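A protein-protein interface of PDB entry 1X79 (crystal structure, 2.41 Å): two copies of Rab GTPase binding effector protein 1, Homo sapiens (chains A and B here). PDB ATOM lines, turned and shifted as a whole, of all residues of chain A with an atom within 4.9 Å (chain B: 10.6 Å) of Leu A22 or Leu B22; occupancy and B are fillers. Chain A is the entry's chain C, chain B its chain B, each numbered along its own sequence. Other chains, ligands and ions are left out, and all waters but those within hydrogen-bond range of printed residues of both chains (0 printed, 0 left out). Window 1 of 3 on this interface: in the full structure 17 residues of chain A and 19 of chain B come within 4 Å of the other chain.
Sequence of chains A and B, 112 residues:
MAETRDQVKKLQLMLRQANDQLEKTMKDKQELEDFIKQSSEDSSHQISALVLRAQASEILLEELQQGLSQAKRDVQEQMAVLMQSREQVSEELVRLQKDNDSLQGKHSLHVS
Of the 17 printed residues of chain B, 5 touch a printed residue of chain A. Of the 9 printed residues of chain A, 4 touch a printed residue of chain B. Hydrophobic or aromatic side chains of chain A that line the printed part of chain B: Ala A18, Leu A22 and Met A26.
Of chain B, only Ala B18 (3.9 Å) comes within 4 Å of Ala A18. No residue of chain B comes within 4 Å of Gln A21. Of chain B, only Leu B22 (3.9 Å) comes within 4 Å of Leu A22. No residue of chain B comes within 4 Å of Glu A23. Of the printed residues of chain B, Met A26 touches Gln B21 and Thr B25. Of the printed residues of chain A, Ala B18 touches Ala A18 (3.9 Å). Of the printed residues of chain A, Gln B21 touches Met A26 (3.6 Å). Of the printed residues of chain A, Thr B25 touches Thr A25 and Met A26. Of the printed residues of chain A, Met B26 touches Thr A25. The nearest residue of chain B that does not touch Leu A22 is Gln B21 (4.1 Å).
Among the printed residues, pairs that only touch across the chains: Thr A25 with Thr B25 (3.3 Å), Thr A25 with Met B26 (3.7 Å), Thr A25 with Leu B22 (3.8 Å), Met A26 with Thr B25 (3.9 Å), Ala A18 with Ala B18 (3.9 Å) and Leu A22 with Leu B22 (3.9 Å).
The side-chain sulfur (SD) of Met A26 sits at hydrogen-bond distance from the side-chain amide nitrogen (NE2) of Gln B21 (3.6 Å).
Ala A18 touches its own counterpart, Ala B18. Thr A25 touches Leu B22, but with the chains exchanged Leu A22 does not touch Thr B25 (4.2 Å). Thr A25 touches Met B26, and with the chains exchanged Met A26 touches Thr B25. Met A26 touches Gln B21, but with the chains exchanged Gln A21 does not touch Met B26 (6.3 Å). Positions printed for both chains: 18, 19, 20, 21, 22, 23, 24, 25 and 26. Of the 7 pairs that touch across the chains among the printed residues, 5 have their exchanged pair printed and touching as well.
The side-chain hydroxyl (OG1) of Thr B25 is in hydrogen-bond range of the backbone carbonyl oxygen (O) of Gln B21. The backbone carbonyl oxygen of Gln A21 lies within hydrogen-bond range of the side-chain hydroxyl of Thr A25, at 3.1 Å.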
ATOM      1  N   ALA A  18      -2.801 -16.238   9.813  1.00  0.00           N
ATOM      2  CA  ALA A  18      -2.821 -17.521   9.128  1.00  0.00           C
ATOM      3  C   ALA A  18      -4.049 -18.276   9.567  1.00  0.00           C
ATOM      4  O   ALA A  18      -4.805 -18.780   8.733  1.00  0.00           O
ATOM      5  CB  ALA A  18      -1.599 -18.328   9.453  1.00  0.00           C
ATOM      6  N   ASN A  19      -4.259 -18.350  10.876  1.00  0.00           N
ATOM      7  CA  ASN A  19      -5.356 -19.148  11.406  1.00  0.00           C
ATOM      8  C   ASN A  19      -6.738 -18.686  10.948  1.00  0.00           C
ATOM      9  O   ASN A  19      -7.561 -19.509  10.620  1.00  0.00           O
ATOM     10  CB  ASN A  19      -5.326 -19.196  12.930  1.00  0.00           C
ATOM     11  CG  ASN A  19      -6.058 -20.423  13.472  1.00  0.00           C
ATOM     12  OD1 ASN A  19      -5.745 -21.563  13.096  1.00  0.00           O
ATOM     13  ND2 ASN A  19      -7.044 -20.201  14.343  1.00  0.00           N
ATOM     14  N   ASP A  20      -6.990 -17.386  10.918  1.00  0.00           N
ATOM     15  CA  ASP A  20      -8.268 -16.892  10.459  1.00  0.00           C
ATOM     16  C   ASP A  20      -8.501 -17.411   9.069  1.00  0.00           C
ATOM     17  O   ASP A  20      -9.627 -17.738   8.697  1.00  0.00           O
ATOM     18  CB  ASP A  20      -8.293 -15.362  10.419  1.00  0.00           C
ATOM     19  CG  ASP A  20      -8.253 -14.745  11.813  1.00  0.00           C
ATOM     20  OD1 ASP A  20      -8.432 -15.510  12.805  1.00  0.00           O
ATOM     21  OD2 ASP A  20      -8.055 -13.506  11.915  1.00  0.00           O
ATOM     22  N   GLN A  21      -7.422 -17.479   8.297  1.00  0.00           N
ATOM     23  CA  GLN A  21      -7.497 -17.786   6.880  1.00  0.00           C
ATOM     24  C   GLN A  21      -7.738 -19.279   6.758  1.00  0.00           C
ATOM     25  O   GLN A  21      -8.626 -19.718   6.063  1.00  0.00           O
ATOM     26  CB  GLN A  21      -6.179 -17.393   6.210  1.00  0.00           C
ATOM     27  CG  GLN A  21      -6.326 -17.054   4.782  1.00  0.00           C
ATOM     28  CD  GLN A  21      -7.248 -15.852   4.593  1.00  0.00           C
ATOM     29  OE1 GLN A  21      -8.072 -15.825   3.672  1.00  0.00           O
ATOM     30  NE2 GLN A  21      -7.106 -14.849   5.459  1.00  0.00           N
ATOM     31  N   LEU A  22      -6.943 -20.052   7.467  1.00  0.00           N
ATOM     32  CA  LEU A  22      -7.151 -21.476   7.556  1.00  0.00           C
ATOM     33  C   LEU A  22      -8.603 -21.808   7.870  1.00  0.00           C
ATOM     34  O   LEU A  22      -9.189 -22.676   7.247  1.00  0.00           O
ATOM     35  CB  LEU A  22      -6.275 -22.059   8.649  1.00  0.00           C
ATOM     36  CG  LEU A  22      -5.466 -23.282   8.276  1.00  0.00           C
ATOM     37  CD1 LEU A  22      -5.062 -23.985   9.548  1.00  0.00           C
ATOM     38  CD2 LEU A  22      -6.281 -24.220   7.422  1.00  0.00           C
ATOM     39  N   GLU A  23      -9.188 -21.117   8.835  1.00  0.00           N
ATOM     40  CA  GLU A  23     -10.487 -21.520   9.343  1.00  0.00           C
ATOM     41  C   GLU A  23     -11.545 -21.270   8.318  1.00  0.00           C
ATOM     42  O   GLU A  23     -12.394 -22.118   8.078  1.00  0.00           O
ATOM     43  CB  GLU A  23     -10.822 -20.770  10.616  1.00  0.00           C
ATOM     44  CG  GLU A  23      -9.784 -21.037  11.679  1.00  0.00           C
ATOM     45  CD  GLU A  23     -10.251 -20.745  13.072  1.00  0.00           C
ATOM     46  OE1 GLU A  23     -10.822 -19.633  13.295  1.00  0.00           O
ATOM     47  OE2 GLU A  23     -10.027 -21.647  13.933  1.00  0.00           O
ATOM     48  N   LYS A  24     -11.475 -20.107   7.696  1.00  0.00           N
ATOM     49  CA  LYS A  24     -12.402 -19.762   6.654  1.00  0.00           C
ATOM     50  C   LYS A  24     -12.340 -20.808   5.553  1.00  0.00           C
ATOM     51  O   LYS A  24     -13.358 -21.274   5.075  1.00  0.00           O
ATOM     52  CB  LYS A  24     -12.069 -18.388   6.103  1.00  0.00           C
ATOM     53  CG  LYS A  24     -13.126 -17.835   5.184  1.00  0.00           C
ATOM     54  CD  LYS A  24     -12.967 -18.314   3.738  1.00  0.00           C
ATOM     55  CE  LYS A  24     -14.107 -17.761   2.865  1.00  0.00           C
ATOM     56  NZ  LYS A  24     -15.439 -17.991   3.528  1.00  0.00           N
ATOM     57  N   THR A  25     -11.139 -21.190   5.166  1.00  0.00           N
ATOM     58  CA  THR A  25     -10.971 -22.137   4.097  1.00  0.00           C
ATOM     59  C   THR A  25     -11.422 -23.532   4.485  1.00  0.00           C
ATOM     60  O   THR A  25     -11.963 -24.253   3.674  1.00  0.00           O
ATOM     61  CB  THR A  25      -9.530 -22.101   3.641  1.00  0.00           C
ATOM     62  OG1 THR A  25      -9.252 -20.753   3.225  1.00  0.00           O
ATOM     63  CG2 THR A  25      -9.284 -23.031   2.451  1.00  0.00           C
ATOM     64  N   MET A  26     -11.261 -23.913   5.735  1.00  0.00           N
ATOM     65  CA  MET A  26     -11.749 -25.212   6.150  1.00  0.00           C
ATOM     66  C   MET A  26     -13.274 -25.247   6.208  1.00  0.00           C
ATOM     67  O   MET A  26     -13.893 -26.266   5.909  1.00  0.00           O
ATOM     68  CB  MET A  26     -11.154 -25.584   7.504  1.00  0.00           C
ATOM     69  CG  MET A  26      -9.747 -26.152   7.381  1.00  0.00           C
ATOM     70  SD  MET A  26      -8.928 -26.599   8.935  1.00  0.00           S
ATOM     71  CE  MET A  26      -9.858 -25.446  10.197  1.00  0.00           C
ATOM     72  N   MET B  14       4.876 -23.594  14.101  1.00  0.00           N
ATOM     73  CA  MET B  14       3.450 -23.498  13.853  1.00  0.00           C
ATOM     74  C   MET B  14       3.182 -22.747  12.578  1.00  0.00           C
ATOM     75  O   MET B  14       2.385 -23.205  11.768  1.00  0.00           O
ATOM     76  CB  MET B  14       2.710 -22.836  15.016  1.00  0.00           C
ATOM     77  CG  MET B  14       2.356 -23.811  16.162  1.00  0.00           C
ATOM     78  SD  MET B  14       1.305 -22.995  17.389  1.00  0.00           S
ATOM     79  CE  MET B  14       0.723 -24.363  18.356  1.00  0.00           C
ATOM     80  N   LEU B  15       3.856 -21.618  12.377  1.00  0.00           N
ATOM     81  CA  LEU B  15       3.566 -20.795  11.204  1.00  0.00           C
ATOM     82  C   LEU B  15       3.767 -21.637   9.949  1.00  0.00           C
ATOM     83  O   LEU B  15       2.926 -21.640   9.064  1.00  0.00           O
ATOM     84  CB  LEU B  15       4.462 -19.564  11.163  1.00  0.00           C
ATOM     85  CG  LEU B  15       4.015 -18.368  10.329  1.00  0.00           C
ATOM     86  CD1 LEU B  15       2.732 -17.805  10.903  1.00  0.00           C
ATOM     87  CD2 LEU B  15       5.077 -17.274  10.362  1.00  0.00           C
ATOM     88  N   ARG B  16       4.859 -22.391   9.866  1.00  0.00           N
ATOM     89  CA  ARG B  16       5.048 -23.230   8.674  1.00  0.00           C
ATOM     90  C   ARG B  16       3.931 -24.279   8.554  1.00  0.00           C
ATOM     91  O   ARG B  16       3.416 -24.532   7.467  1.00  0.00           O
ATOM     92  CB  ARG B  16       6.439 -23.897   8.684  1.00  0.00           C
ATOM     93  CG  ARG B  16       6.566 -25.163   7.824  1.00  0.00           C
ATOM     94  CD  ARG B  16       6.458 -24.931   6.331  1.00  0.00           C
ATOM     95  NE  ARG B  16       7.420 -23.936   5.899  1.00  0.00           N
ATOM     96  CZ  ARG B  16       7.651 -23.632   4.631  1.00  0.00           C
ATOM     97  NH1 ARG B  16       6.983 -24.252   3.668  1.00  0.00           N
ATOM     98  NH2 ARG B  16       8.554 -22.710   4.327  1.00  0.00           N
ATOM     99  N   GLN B  17       3.549 -24.866   9.675  1.00  0.00           N
ATOM    100  CA  GLN B  17       2.440 -25.808   9.709  1.00  0.00           C
ATOM    101  C   GLN B  17       1.129 -25.188   9.256  1.00  0.00           C
ATOM    102  O   GLN B  17       0.390 -25.788   8.509  1.00  0.00           O
ATOM    103  CB  GLN B  17       2.277 -26.374  11.114  1.00  0.00           C
ATOM    104  CG  GLN B  17       3.415 -27.293  11.483  1.00  0.00           C
ATOM    105  CD  GLN B  17       3.312 -27.860  12.892  1.00  0.00           C
ATOM    106  OE1 GLN B  17       2.743 -27.238  13.797  1.00  0.00           O
ATOM    107  NE2 GLN B  17       3.891 -29.039  13.088  1.00  0.00           N
ATOM    108  N   ALA B  18       0.837 -23.980   9.693  1.00  0.00           N
ATOM    109  CA  ALA B  18      -0.364 -23.353   9.206  1.00  0.00           C
ATOM    110  C   ALA B  18      -0.274 -23.130   7.693  1.00  0.00           C
ATOM    111  O   ALA B  18      -1.224 -23.408   6.961  1.00  0.00           O
ATOM    112  CB  ALA B  18      -0.583 -22.063   9.917  1.00  0.00           C
ATOM    113  N   ASN B  19       0.871 -22.647   7.220  1.00  0.00           N
ATOM    114  CA  ASN B  19       1.065 -22.449   5.798  1.00  0.00           C
ATOM    115  C   ASN B  19       0.788 -23.738   5.040  1.00  0.00           C
ATOM    116  O   ASN B  19       0.026 -23.753   4.075  1.00  0.00           O
ATOM    117  CB  ASN B  19       2.491 -22.023   5.513  1.00  0.00           C
ATOM    118  CG  ASN B  19       2.789 -21.960   4.027  1.00  0.00           C
ATOM    119  OD1 ASN B  19       2.449 -20.993   3.354  1.00  0.00           O
ATOM    120  ND2 ASN B  19       3.424 -22.995   3.511  1.00  0.00           N
ATOM    121  N   ASP B  20       1.398 -24.833   5.481  1.00  0.00           N
ATOM    122  CA  ASP B  20       1.232 -26.086   4.767  1.00  0.00           C
ATOM    123  C   ASP B  20      -0.206 -26.546   4.778  1.00  0.00           C
ATOM    124  O   ASP B  20      -0.719 -27.036   3.762  1.00  0.00           O
ATOM    125  CB  ASP B  20       2.125 -27.155   5.355  1.00  0.00           C
ATOM    126  CG  ASP B  20       3.596 -26.906   5.040  1.00  0.00           C
ATOM    127  OD1 ASP B  20       3.934 -25.981   4.239  1.00  0.00           O
ATOM    128  OD2 ASP B  20       4.421 -27.657   5.589  1.00  0.00           O
ATOM    129  N   GLN B  21      -0.874 -26.365   5.910  1.00  0.00           N
ATOM    130  CA  GLN B  21      -2.224 -26.827   5.985  1.00  0.00           C
ATOM    131  C   GLN B  21      -3.168 -25.928   5.183  1.00  0.00           C
ATOM    132  O   GLN B  21      -4.082 -26.423   4.518  1.00  0.00           O
ATOM    133  CB  GLN B  21      -2.661 -26.908   7.415  1.00  0.00           C
ATOM    134  CG  GLN B  21      -3.810 -27.840   7.551  1.00  0.00           C
ATOM    135  CD  GLN B  21      -4.274 -27.981   8.970  1.00  0.00           C
ATOM    136  OE1 GLN B  21      -3.456 -28.041   9.907  1.00  0.00           O
ATOM    137  NE2 GLN B  21      -5.595 -28.054   9.149  1.00  0.00           N
ATOM    138  N   LEU B  22      -2.933 -24.619   5.207  1.00  0.00           N
ATOM    139  CA  LEU B  22      -3.770 -23.713   4.423  1.00  0.00           C
ATOM    140  C   LEU B  22      -3.621 -24.126   2.968  1.00  0.00           C
ATOM    141  O   LEU B  22      -4.572 -24.100   2.205  1.00  0.00           O
ATOM    142  CB  LEU B  22      -3.314 -22.269   4.574  1.00  0.00           C
ATOM    143  CG  LEU B  22      -4.214 -21.036   4.336  1.00  0.00           C
ATOM    144  CD1 LEU B  22      -3.448 -19.979   3.526  1.00  0.00           C
ATOM    145  CD2 LEU B  22      -5.506 -21.433   3.632  1.00  0.00           C
ATOM    146  N   GLU B  23      -2.416 -24.530   2.590  1.00  0.00           N
ATOM    147  CA  GLU B  23      -2.140 -24.879   1.206  1.00  0.00           C
ATOM    148  C   GLU B  23      -2.883 -26.129   0.774  1.00  0.00           C
ATOM    149  O   GLU B  23      -3.499 -26.143  -0.286  1.00  0.00           O
ATOM    150  CB  GLU B  23      -0.661 -25.092   1.021  1.00  0.00           C
ATOM    151  CG  GLU B  23      -0.274 -25.508  -0.330  1.00  0.00           C
ATOM    152  CD  GLU B  23       1.220 -25.572  -0.479  1.00  0.00           C
ATOM    153  OE1 GLU B  23       1.808 -26.649  -0.234  1.00  0.00           O
ATOM    154  OE2 GLU B  23       1.808 -24.525  -0.822  1.00  0.00           O
ATOM    155  N   LYS B  24      -2.829 -27.179   1.583  1.00  0.00           N
ATOM    156  CA  LYS B  24      -3.540 -28.385   1.247  1.00  0.00           C
ATOM    157  C   LYS B  24      -5.026 -28.076   1.254  1.00  0.00           C
ATOM    158  O   LYS B  24      -5.769 -28.488   0.367  1.00  0.00           O
ATOM    159  CB  LYS B  24      -3.285 -29.500   2.253  1.00  0.00           C
ATOM    160  CG  LYS B  24      -3.794 -30.856   1.741  1.00  0.00           C
ATOM    161  CD  LYS B  24      -3.887 -31.897   2.831  1.00  0.00           C
ATOM    162  CE  LYS B  24      -5.105 -31.653   3.722  1.00  0.00           C
ATOM    163  NZ  LYS B  24      -4.896 -32.177   5.125  1.00  0.00           N
ATOM    164  N   THR B  25      -5.481 -27.359   2.257  1.00  0.00           N
ATOM    165  CA  THR B  25      -6.904 -27.160   2.324  1.00  0.00           C
ATOM    166  C   THR B  25      -7.376 -26.397   1.106  1.00  0.00           C
ATOM    167  O   THR B  25      -8.458 -26.678   0.593  1.00  0.00           O
ATOM    168  CB  THR B  25      -7.292 -26.429   3.609  1.00  0.00           C
ATOM    169  OG1 THR B  25      -7.016 -27.295   4.715  1.00  0.00           O
ATOM    170  CG2 THR B  25      -8.783 -26.069   3.612  1.00  0.00           C
ATOM    171  N   MET B  26      -6.577 -25.452   0.614  1.00  0.00           N
ATOM    172  CA  MET B  26      -7.024 -24.678  -0.543  1.00  0.00           C
ATOM    173  C   MET B  26      -7.024 -25.542  -1.810  1.00  0.00           C
ATOM    174  O   MET B  26      -7.913 -25.432  -2.658  1.00  0.00           O
ATOM    175  CB  MET B  26      -6.146 -23.445  -0.744  1.00  0.00           C
ATOM    176  CG  MET B  26      -6.430 -22.326   0.213  1.00  0.00           C
ATOM    177  SD  MET B  26      -5.152 -21.036   0.106  1.00  0.00           S
ATOM    178  CE  MET B  26      -5.274 -20.693  -1.557  1.00  0.00           C
ATOM    179  N   LYS B  27      -6.022 -26.406  -1.920  1.00  0.00           N
ATOM    180  CA  LYS B  27      -5.958 -27.400  -2.983  1.00  0.00           C
ATOM    181  C   LYS B  27      -7.184 -28.314  -2.948  1.00  0.00           C
ATOM    182  O   LYS B  27      -7.864 -28.477  -3.949  1.00  0.00           O
ATOM    183  CB  LYS B  27      -4.687 -28.238  -2.835  1.00  0.00           C
ATOM    184  CG  LYS B  27      -4.508 -29.341  -3.865  1.00  0.00           C
ATOM    185  CD  LYS B  27      -3.437 -30.334  -3.439  1.00  0.00           C
ATOM    186  CE  LYS B  27      -2.898 -31.106  -4.627  1.00  0.00           C
ATOM    187  NZ  LYS B  27      -2.118 -30.243  -5.584  1.00  0.00           N
ATOM    188  N   ASP B  28      -7.468 -28.906  -1.794  1.00  0.00           N
ATOM    189  CA  ASP B  28      -8.668 -29.728  -1.642  1.00  0.00           C
ATOM    190  C   ASP B  28      -9.953 -28.970  -2.022  1.00  0.00           C
ATOM    191  O   ASP B  28     -10.772 -29.468  -2.762  1.00  0.00           O
ATOM    192  CB  ASP B  28      -8.800 -30.236  -0.199  1.00  0.00           C
ATOM    193  CG  ASP B  28      -7.700 -31.206   0.192  1.00  0.00           C
ATOM    194  OD1 ASP B  28      -6.931 -31.635  -0.689  1.00  0.00           O
ATOM    195  OD2 ASP B  28      -7.608 -31.533   1.397  1.00  0.00           O
ATOM    196  N   LYS B  29     -10.137 -27.771  -1.503  1.00  0.00           N
ATOM    197  CA  LYS B  29     -11.329 -27.024  -1.819  1.00  0.00           C
ATOM    198  C   LYS B  29     -11.478 -26.957  -3.329  1.00  0.00           C
ATOM    199  O   LYS B  29     -12.580 -27.060  -3.842  1.00  0.00           O
ATOM    200  CB  LYS B  29     -11.218 -25.622  -1.264  1.00  0.00           C
ATOM    201  CG  LYS B  29     -12.473 -24.812  -1.352  1.00  0.00           C
ATOM    202  CD  LYS B  29     -12.144 -23.373  -1.103  1.00  0.00           C
ATOM    203  CE  LYS B  29     -13.323 -22.457  -1.257  1.00  0.00           C
ATOM    204  NZ  LYS B  29     -12.840 -21.085  -0.981  1.00  0.00           N
ATOM    205  N   GLN B  30     -10.375 -26.787  -4.047  1.00  0.00           N
ATOM    206  CA  GLN B  30     -10.448 -26.593  -5.489  1.00  0.00           C
ATOM    207  C   GLN B  30     -10.856 -27.898  -6.166  1.00  0.00           C
ATOM    208  O   GLN B  30     -11.751 -27.933  -7.023  1.00  0.00           O
ATOM    209  CB  GLN B  30      -9.097 -26.134  -6.043  1.00  0.00           C
ATOM    210  CG  GLN B  30      -9.090 -25.922  -7.561  1.00  0.00           C
ATOM    211  CD  GLN B  30      -9.969 -24.747  -7.989  1.00  0.00           C
ATOM    212  OE1 GLN B  30      -9.695 -23.583  -7.642  1.00  0.00           O
ATOM    213  NE2 GLN B  30     -11.040 -25.047  -8.741  1.00  0.00           N
